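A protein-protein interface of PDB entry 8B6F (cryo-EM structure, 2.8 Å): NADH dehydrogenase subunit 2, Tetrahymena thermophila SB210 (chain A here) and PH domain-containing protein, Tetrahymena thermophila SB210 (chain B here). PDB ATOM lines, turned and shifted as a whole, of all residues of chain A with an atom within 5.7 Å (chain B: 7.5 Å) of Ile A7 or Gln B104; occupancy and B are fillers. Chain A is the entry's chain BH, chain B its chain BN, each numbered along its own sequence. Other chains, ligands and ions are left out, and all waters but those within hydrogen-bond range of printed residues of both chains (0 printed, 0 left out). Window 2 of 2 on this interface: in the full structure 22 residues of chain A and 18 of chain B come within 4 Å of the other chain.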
ATOM      1  N   SER A   2      -0.421  -2.887  -4.887  1.00  0.00           N
ATOM      2  CA  SER A   2      -0.318  -1.850  -5.900  1.00  0.00           C
ATOM      3  C   SER A   2      -1.230  -2.191  -7.067  1.00  0.00           C
ATOM      4  O   SER A   2      -1.432  -3.363  -7.392  1.00  0.00           O
ATOM      5  CB  SER A   2       1.123  -1.692  -6.399  1.00  0.00           C
ATOM      6  OG  SER A   2       2.006  -1.398  -5.330  1.00  0.00           O
ATOM      7  N   ILE A   3      -1.778  -1.155  -7.696  1.00  0.00           N
ATOM      8  CA  ILE A   3      -2.707  -1.305  -8.809  1.00  0.00           C
ATOM      9  C   ILE A   3      -2.072  -0.677 -10.041  1.00  0.00           C
ATOM     10  O   ILE A   3      -1.681   0.496 -10.014  1.00  0.00           O
ATOM     11  CB  ILE A   3      -4.065  -0.643  -8.514  1.00  0.00           C
ATOM     12  CG1 ILE A   3      -4.527  -0.976  -7.094  1.00  0.00           C
ATOM     13  CG2 ILE A   3      -5.096  -1.113  -9.529  1.00  0.00           C
ATOM     14  CD1 ILE A   3      -5.831  -0.309  -6.701  1.00  0.00           C
ATOM     15  N   PHE A   4      -1.973  -1.453 -11.116  1.00  0.00           N
ATOM     16  CA  PHE A   4      -1.449  -0.979 -12.395  1.00  0.00           C
ATOM     17  C   PHE A   4      -2.396  -1.467 -13.485  1.00  0.00           C
ATOM     18  O   PHE A   4      -2.291  -2.609 -13.941  1.00  0.00           O
ATOM     19  CB  PHE A   4      -0.025  -1.474 -12.630  1.00  0.00           C
ATOM     20  CG  PHE A   4       0.961  -0.999 -11.601  1.00  0.00           C
ATOM     21  CD1 PHE A   4       1.584   0.229 -11.735  1.00  0.00           C
ATOM     22  CD2 PHE A   4       1.264  -1.781 -10.504  1.00  0.00           C
ATOM     23  CE1 PHE A   4       2.493   0.666 -10.791  1.00  0.00           C
ATOM     24  CE2 PHE A   4       2.172  -1.349  -9.556  1.00  0.00           C
ATOM     25  CZ  PHE A   4       2.785  -0.124  -9.699  1.00  0.00           C
ATOM     26  N   SER A   5      -3.315  -0.600 -13.905  1.00  0.00           N
ATOM     27  CA  SER A   5      -4.324  -0.955 -14.900  1.00  0.00           C
ATOM     28  C   SER A   5      -5.144  -2.155 -14.431  1.00  0.00           C
ATOM     29  O   SER A   5      -5.325  -3.138 -15.152  1.00  0.00           O
ATOM     30  CB  SER A   5      -3.677  -1.230 -16.259  1.00  0.00           C
ATOM     31  OG  SER A   5      -4.656  -1.544 -17.236  1.00  0.00           O
ATOM     32  N   ASN A   6      -5.641  -2.067 -13.198  1.00  0.00           N
ATOM     33  CA  ASN A   6      -6.504  -3.077 -12.599  1.00  0.00           C
ATOM     34  C   ASN A   6      -5.788  -4.399 -12.358  1.00  0.00           C
ATOM     35  O   ASN A   6      -6.442  -5.432 -12.189  1.00  0.00           O
ATOM     36  CB  ASN A   6      -7.749  -3.314 -13.460  1.00  0.00           C
ATOM     37  CG  ASN A   6      -8.456  -2.025 -13.821  1.00  0.00           C
ATOM     38  OD1 ASN A   6      -9.307  -1.542 -13.075  1.00  0.00           O
ATOM     39  ND2 ASN A   6      -8.107  -1.459 -14.971  1.00  0.00           N
ATOM     40  N   ILE A   7      -4.459  -4.397 -12.342  1.00  0.00           N
ATOM     41  CA  ILE A   7      -3.665  -5.571 -11.994  1.00  0.00           C
ATOM     42  C   ILE A   7      -3.087  -5.339 -10.608  1.00  0.00           C
ATOM     43  O   ILE A   7      -2.280  -4.421 -10.410  1.00  0.00           O
ATOM     44  CB  ILE A   7      -2.555  -5.841 -13.025  1.00  0.00           C
ATOM     45  CG1 ILE A   7      -3.093  -6.648 -14.209  1.00  0.00           C
ATOM     46  CG2 ILE A   7      -1.384  -6.596 -12.400  1.00  0.00           C
ATOM     47  CD1 ILE A   7      -4.129  -5.929 -15.032  1.00  0.00           C
ATOM     48  N   TRP A   8      -3.502  -6.159  -9.649  1.00  0.00           N
ATOM     49  CA  TRP A   8      -3.009  -6.037  -8.286  1.00  0.00           C
ATOM     50  C   TRP A   8      -1.659  -6.723  -8.143  1.00  0.00           C
ATOM     51  O   TRP A   8      -1.437  -7.811  -8.680  1.00  0.00           O
ATOM     52  CB  TRP A   8      -3.996  -6.654  -7.301  1.00  0.00           C
ATOM     53  CG  TRP A   8      -5.288  -5.942  -7.255  1.00  0.00           C
ATOM     54  CD1 TRP A   8      -6.363  -6.170  -8.052  1.00  0.00           C
ATOM     55  CD2 TRP A   8      -5.660  -4.883  -6.366  1.00  0.00           C
ATOM     56  NE1 TRP A   8      -7.382  -5.324  -7.720  1.00  0.00           N
ATOM     57  CE2 TRP A   8      -6.978  -4.518  -6.687  1.00  0.00           C
ATOM     58  CE3 TRP A   8      -5.004  -4.207  -5.333  1.00  0.00           C
ATOM     59  CZ2 TRP A   8      -7.658  -3.509  -6.012  1.00  0.00           C
ATOM     60  CZ3 TRP A   8      -5.679  -3.204  -4.663  1.00  0.00           C
ATOM     61  CH2 TRP A   8      -6.994  -2.865  -5.005  1.00  0.00           C
ATOM     62  N   ILE A   9      -0.753  -6.076  -7.417  1.00  0.00           N
ATOM     63  CA  ILE A   9       0.568  -6.618  -7.134  1.00  0.00           C
ATOM     64  C   ILE A   9       0.767  -6.586  -5.628  1.00  0.00           C
ATOM     65  O   ILE A   9       0.616  -5.533  -5.000  1.00  0.00           O
ATOM     66  CB  ILE A   9       1.680  -5.831  -7.850  1.00  0.00           C
ATOM     67  CG1 ILE A   9       1.404  -5.804  -9.355  1.00  0.00           C
ATOM     68  CG2 ILE A   9       3.040  -6.448  -7.550  1.00  0.00           C
ATOM     69  CD1 ILE A   9       2.399  -5.002 -10.150  1.00  0.00           C
ATOM     70  N   ASN A  11       3.519  -7.537  -2.779  1.00  0.00           N
ATOM     71  CA  ASN A  11       4.865  -7.900  -2.367  1.00  0.00           C
ATOM     72  C   ASN A  11       4.951  -8.202  -0.878  1.00  0.00           C
ATOM     73  O   ASN A  11       6.057  -8.343  -0.348  1.00  0.00           O
ATOM     74  CB  ASN A  11       5.845  -6.783  -2.723  1.00  0.00           C
ATOM     75  CG  ASN A  11       5.866  -6.475  -4.205  1.00  0.00           C
ATOM     76  OD1 ASN A  11       5.534  -7.323  -5.032  1.00  0.00           O
ATOM     77  ND2 ASN A  11       6.260  -5.255  -4.549  1.00  0.00           N
ATOM     78  N   ARG B  92       7.551 -16.989  -2.990  1.00  0.00           N
ATOM     79  CA  ARG B  92       7.574 -17.031  -4.446  1.00  0.00           C
ATOM     80  C   ARG B  92       8.524 -15.985  -5.009  1.00  0.00           C
ATOM     81  O   ARG B  92       9.154 -16.211  -6.046  1.00  0.00           O
ATOM     82  CB  ARG B  92       6.169 -16.812  -5.003  1.00  0.00           C
ATOM     83  CG  ARG B  92       5.270 -18.035  -4.958  1.00  0.00           C
ATOM     84  CD  ARG B  92       3.898 -17.707  -5.518  1.00  0.00           C
ATOM     85  NE  ARG B  92       3.981 -17.217  -6.887  1.00  0.00           N
ATOM     86  CZ  ARG B  92       2.988 -16.623  -7.536  1.00  0.00           C
ATOM     87  NH1 ARG B  92       1.814 -16.416  -6.964  1.00  0.00           N
ATOM     88  NH2 ARG B  92       3.180 -16.225  -8.789  1.00  0.00           N
ATOM     89  N   LEU B  93       8.621 -14.826  -4.358  1.00  0.00           N
ATOM     90  CA  LEU B  93       9.570 -13.814  -4.804  1.00  0.00           C
ATOM     91  C   LEU B  93      10.997 -14.173  -4.403  1.00  0.00           C
ATOM     92  O   LEU B  93      11.938 -13.908  -5.157  1.00  0.00           O
ATOM     93  CB  LEU B  93       9.181 -12.450  -4.229  1.00  0.00           C
ATOM     94  CG  LEU B  93      10.088 -11.266  -4.568  1.00  0.00           C
ATOM     95  CD1 LEU B  93      10.240 -11.105  -6.070  1.00  0.00           C
ATOM     96  CD2 LEU B  93       9.540  -9.993  -3.948  1.00  0.00           C
ATOM     97  N   GLU B  98      11.322 -15.563 -11.343  1.00  0.00           N
ATOM     98  CA  GLU B  98      10.867 -15.461 -12.726  1.00  0.00           C
ATOM     99  C   GLU B  98       9.395 -15.827 -12.847  1.00  0.00           C
ATOM    100  O   GLU B  98       8.630 -15.141 -13.534  1.00  0.00           O
ATOM    101  CB  GLU B  98      11.711 -16.360 -13.629  1.00  0.00           C
ATOM    102  CG  GLU B  98      13.155 -15.923 -13.783  1.00  0.00           C
ATOM    103  CD  GLU B  98      14.004 -16.250 -12.572  1.00  0.00           C
ATOM    104  OE1 GLU B  98      13.438 -16.659 -11.538  1.00  0.00           O
ATOM    105  OE2 GLU B  98      15.241 -16.103 -12.651  1.00  0.00           O
ATOM    106  N   ILE B  99       8.982 -16.915 -12.195  1.00  0.00           N
ATOM    107  CA  ILE B  99       7.579 -17.320 -12.235  1.00  0.00           C
ATOM    108  C   ILE B  99       6.708 -16.271 -11.558  1.00  0.00           C
ATOM    109  O   ILE B  99       5.597 -15.974 -12.012  1.00  0.00           O
ATOM    110  CB  ILE B  99       7.407 -18.707 -11.589  1.00  0.00           C
ATOM    111  CG1 ILE B  99       8.184 -19.756 -12.388  1.00  0.00           C
ATOM    112  CG2 ILE B  99       5.931 -19.087 -11.514  1.00  0.00           C
ATOM    113  CD1 ILE B  99       8.298 -21.094 -11.696  1.00  0.00           C
ATOM    114  N   PHE B 100       7.195 -15.701 -10.455  1.00  0.00           N
ATOM    115  CA  PHE B 100       6.460 -14.640  -9.775  1.00  0.00           C
ATOM    116  C   PHE B 100       6.212 -13.465 -10.713  1.00  0.00           C
ATOM    117  O   PHE B 100       5.088 -12.961 -10.812  1.00  0.00           O
ATOM    118  CB  PHE B 100       7.238 -14.199  -8.534  1.00  0.00           C
ATOM    119  CG  PHE B 100       6.551 -13.135  -7.729  1.00  0.00           C
ATOM    120  CD1 PHE B 100       5.567 -13.468  -6.814  1.00  0.00           C
ATOM    121  CD2 PHE B 100       6.910 -11.805  -7.864  1.00  0.00           C
ATOM    122  CE1 PHE B 100       4.940 -12.494  -6.064  1.00  0.00           C
ATOM    123  CE2 PHE B 100       6.288 -10.827  -7.115  1.00  0.00           C
ATOM    124  CZ  PHE B 100       5.301 -11.172  -6.215  1.00  0.00           C
ATOM    125  N   LEU B 101       7.257 -13.012 -11.407  1.00  0.00           N
ATOM    126  CA  LEU B 101       7.109 -11.883 -12.320  1.00  0.00           C
ATOM    127  C   LEU B 101       6.185 -12.221 -13.483  1.00  0.00           C
ATOM    128  O   LEU B 101       5.363 -11.393 -13.892  1.00  0.00           O
ATOM    129  CB  LEU B 101       8.481 -11.448 -12.834  1.00  0.00           C
ATOM    130  CG  LEU B 101       9.433 -10.879 -11.780  1.00  0.00           C
ATOM    131  CD1 LEU B 101      10.804 -10.636 -12.381  1.00  0.00           C
ATOM    132  CD2 LEU B 101       8.882  -9.597 -11.182  1.00  0.00           C
ATOM    133  N   ARG B 102       6.306 -13.430 -14.036  1.00  0.00           N
ATOM    134  CA  ARG B 102       5.462 -13.810 -15.165  1.00  0.00           C
ATOM    135  C   ARG B 102       3.995 -13.891 -14.756  1.00  0.00           C
ATOM    136  O   ARG B 102       3.115 -13.458 -15.506  1.00  0.00           O
ATOM    137  CB  ARG B 102       5.934 -15.134 -15.760  1.00  0.00           C
ATOM    138  CG  ARG B 102       5.213 -15.501 -17.047  1.00  0.00           C
ATOM    139  CD  ARG B 102       6.106 -16.273 -18.004  1.00  0.00           C
ATOM    140  NE  ARG B 102       7.261 -15.490 -18.426  1.00  0.00           N
ATOM    141  CZ  ARG B 102       8.156 -15.893 -19.317  1.00  0.00           C
ATOM    142  NH1 ARG B 102       8.050 -17.066 -19.921  1.00  0.00           N
ATOM    143  NH2 ARG B 102       9.185 -15.103 -19.607  1.00  0.00           N
ATOM    144  N   ASP B 103       3.709 -14.452 -13.578  1.00  0.00           N
ATOM    145  CA  ASP B 103       2.336 -14.455 -13.083  1.00  0.00           C
ATOM    146  C   ASP B 103       1.826 -13.034 -12.901  1.00  0.00           C
ATOM    147  O   ASP B 103       0.682 -12.722 -13.251  1.00  0.00           O
ATOM    148  CB  ASP B 103       2.248 -15.215 -11.759  1.00  0.00           C
ATOM    149  CG  ASP B 103       2.518 -16.695 -11.912  1.00  0.00           C
ATOM    150  OD1 ASP B 103       2.156 -17.262 -12.964  1.00  0.00           O
ATOM    151  OD2 ASP B 103       3.094 -17.297 -10.982  1.00  0.00           O
ATOM    152  N   GLN B 104       2.668 -12.159 -12.355  1.00  0.00           N
ATOM    153  CA  GLN B 104       2.301 -10.758 -12.196  1.00  0.00           C
ATOM    154  C   GLN B 104       2.005 -10.101 -13.537  1.00  0.00           C
ATOM    155  O   GLN B 104       1.140  -9.221 -13.618  1.00  0.00           O
ATOM    156  CB  GLN B 104       3.426 -10.032 -11.466  1.00  0.00           C
ATOM    157  CG  GLN B 104       3.253  -8.541 -11.326  1.00  0.00           C
ATOM    158  CD  GLN B 104       4.441  -7.921 -10.633  1.00  0.00           C
ATOM    159  OE1 GLN B 104       5.050  -6.977 -11.137  1.00  0.00           O
ATOM    160  NE2 GLN B 104       4.789  -8.461  -9.472  1.00  0.00           N
ATOM    161  N   GLN B 105       2.704 -10.506 -14.595  1.00  0.00           N
ATOM    162  CA  GLN B 105       2.577  -9.894 -15.910  1.00  0.00           C
ATOM    163  C   GLN B 105       1.619 -10.643 -16.822  1.00  0.00           C
ATOM    164  O   GLN B 105       1.525 -10.307 -18.005  1.00  0.00           O
ATOM    165  CB  GLN B 105       3.947  -9.813 -16.584  1.00  0.00           C
ATOM    166  CG  GLN B 105       4.926  -8.938 -15.858  1.00  0.00           C
ATOM    167  CD  GLN B 105       6.331  -9.058 -16.398  1.00  0.00           C
ATOM    168  OE1 GLN B 105       6.560  -9.691 -17.427  1.00  0.00           O
ATOM    169  NE2 GLN B 105       7.284  -8.445 -15.706  1.00  0.00           N
ATOM    170  N   ALA B 106       0.918 -11.653 -16.305  1.00  0.00           N
ATOM    171  CA  ALA B 106       0.050 -12.488 -17.126  1.00  0.00           C
ATOM    172  C   ALA B 106      -0.734 -11.692 -18.165  1.00  0.00           C
ATOM    173  O   ALA B 106      -0.647 -11.964 -19.368  1.00  0.00           O
ATOM    174  CB  ALA B 106      -0.907 -13.267 -16.221  1.00  0.00           C
ATOM    175  N   LYS B 107      -1.516 -10.707 -17.717  1.00  0.00           N
ATOM    176  CA  LYS B 107      -2.350  -9.962 -18.655  1.00  0.00           C
ATOM    177  C   LYS B 107      -1.512  -9.065 -19.556  1.00  0.00           C
ATOM    178  O   LYS B 107      -1.836  -8.885 -20.734  1.00  0.00           O
ATOM    179  CB  LYS B 107      -3.389  -9.137 -17.898  1.00  0.00           C
ATOM    180  CG  LYS B 107      -4.636  -8.846 -18.717  1.00  0.00           C
ATOM    181  CD  LYS B 107      -5.601  -7.942 -17.971  1.00  0.00           C
ATOM    182  CE  LYS B 107      -5.347  -6.474 -18.272  1.00  0.00           C
ATOM    183  NZ  LYS B 107      -5.719  -6.122 -19.670  1.00  0.00           N
ATOM    184  N   PHE B 108      -0.440  -8.479 -19.020  1.00  0.00           N
ATOM    185  CA  PHE B 108       0.425  -7.645 -19.845  1.00  0.00           C
ATOM    186  C   PHE B 108       1.039  -8.435 -20.992  1.00  0.00           C
ATOM    187  O   PHE B 108       1.321  -7.868 -22.053  1.00  0.00           O
ATOM    188  CB  PHE B 108       1.520  -7.014 -18.986  1.00  0.00           C
ATOM    189  CG  PHE B 108       0.999  -6.136 -17.882  1.00  0.00           C
ATOM    190  CD1 PHE B 108      -0.196  -5.446 -18.025  1.00  0.00           C
ATOM    191  CD2 PHE B 108       1.705  -6.002 -16.700  1.00  0.00           C
ATOM    192  CE1 PHE B 108      -0.672  -4.640 -17.009  1.00  0.00           C
ATOM    193  CE2 PHE B 108       1.234  -5.198 -15.681  1.00  0.00           C
ATOM    194  CZ  PHE B 108       0.042  -4.516 -15.836  1.00  0.00           C
ATOM    195  N   ILE B 109       1.251  -9.739 -20.803  1.00  0.00           N
ATOM    196  CA  ILE B 109       1.798 -10.563 -21.878  1.00  0.00           C
ATOM    197  C   ILE B 109       0.837 -10.597 -23.058  1.00  0.00           C
ATOM    198  O   ILE B 109       1.239 -10.416 -24.212  1.00  0.00           O
ATOM    199  CB  ILE B 109       2.113 -11.981 -21.365  1.00  0.00           C
ATOM    200  CG1 ILE B 109       3.181 -11.946 -20.266  1.00  0.00           C
ATOM    201  CG2 ILE B 109       2.565 -12.882 -22.513  1.00  0.00           C
ATOM    202  CD1 ILE B 109       4.528 -11.408 -20.702  1.00  0.00           C
ATOM    203  N   LEU B 111      -1.566  -8.436 -23.689  1.00  0.00           N
ATOM    204  CA  LEU B 111      -1.650  -7.089 -24.241  1.00  0.00           C
ATOM    205  C   LEU B 111      -0.489  -6.822 -25.188  1.00  0.00           C
ATOM    206  O   LEU B 111      -0.675  -6.260 -26.272  1.00  0.00           O
ATOM    207  CB  LEU B 111      -1.671  -6.058 -23.114  1.00  0.00           C
ATOM    208  CG  LEU B 111      -2.955  -5.976 -22.286  1.00  0.00           C
ATOM    209  CD1 LEU B 111      -2.760  -5.037 -21.109  1.00  0.00           C
ATOM    210  CD2 LEU B 111      -4.128  -5.524 -23.137  1.00  0.00           C
ATOM    211  N   LEU B 133       8.088  -6.233 -22.284  1.00  0.00           N
ATOM    212  CA  LEU B 133       8.568  -7.003 -21.147  1.00  0.00           C
ATOM    213  C   LEU B 133       9.547  -8.074 -21.607  1.00  0.00           C
ATOM    214  O   LEU B 133       9.360  -8.692 -22.658  1.00  0.00           O
ATOM    215  CB  LEU B 133       7.395  -7.654 -20.413  1.00  0.00           C
ATOM    216  CG  LEU B 133       6.254  -6.709 -20.030  1.00  0.00           C
ATOM    217  CD1 LEU B 133       5.057  -7.495 -19.533  1.00  0.00           C
ATOM    218  CD2 LEU B 133       6.711  -5.712 -18.979  1.00  0.00           C
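O of Ser A2 sits at hydrogen-bond distance from N of Ile A9, at 2.8 Å.
Among the printed residues, merely in contact across the chains: Ile A9 with Gln B104 (3.3 Å), Ile A7 with Lys B107 (3.5 Å), Phe A4 with Phe B108 (3.6 Å) and Ile A7 with Gln B104 (3.8 Å).
Of the printed residues of chain B, Phe A4 touches Phe B108 (3.6 Å). Ile A7 touches just these residues of chain B: Gln B104 and Lys B107. Of the printed residues of chain B, Ile A9 touches Gln B104 (3.3 Å). Of chain A, only Ile A7 and Ile A9 come within 4 Å of Gln B104. Of the printed residues of chain A, Lys B107 touches Ile A7. Of the printed residues of chain A, Phe B108 touches Phe A4. The nearest residue of chain A that does not touch Gln B104 is Asn A11 (4.6 Å).
Hydrophobic or aromatic side chains of chain B within 4 Å of the printed part of chain A: Phe B108. Printed residues of chain A that touch a printed residue of chain B: Phe A4, Ile A7 and Ile A9. Among the printed residues, no Asp or Glu carboxylate lies within 4 Å of a Lys or Arg side-chain nitrogen of the other chain.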
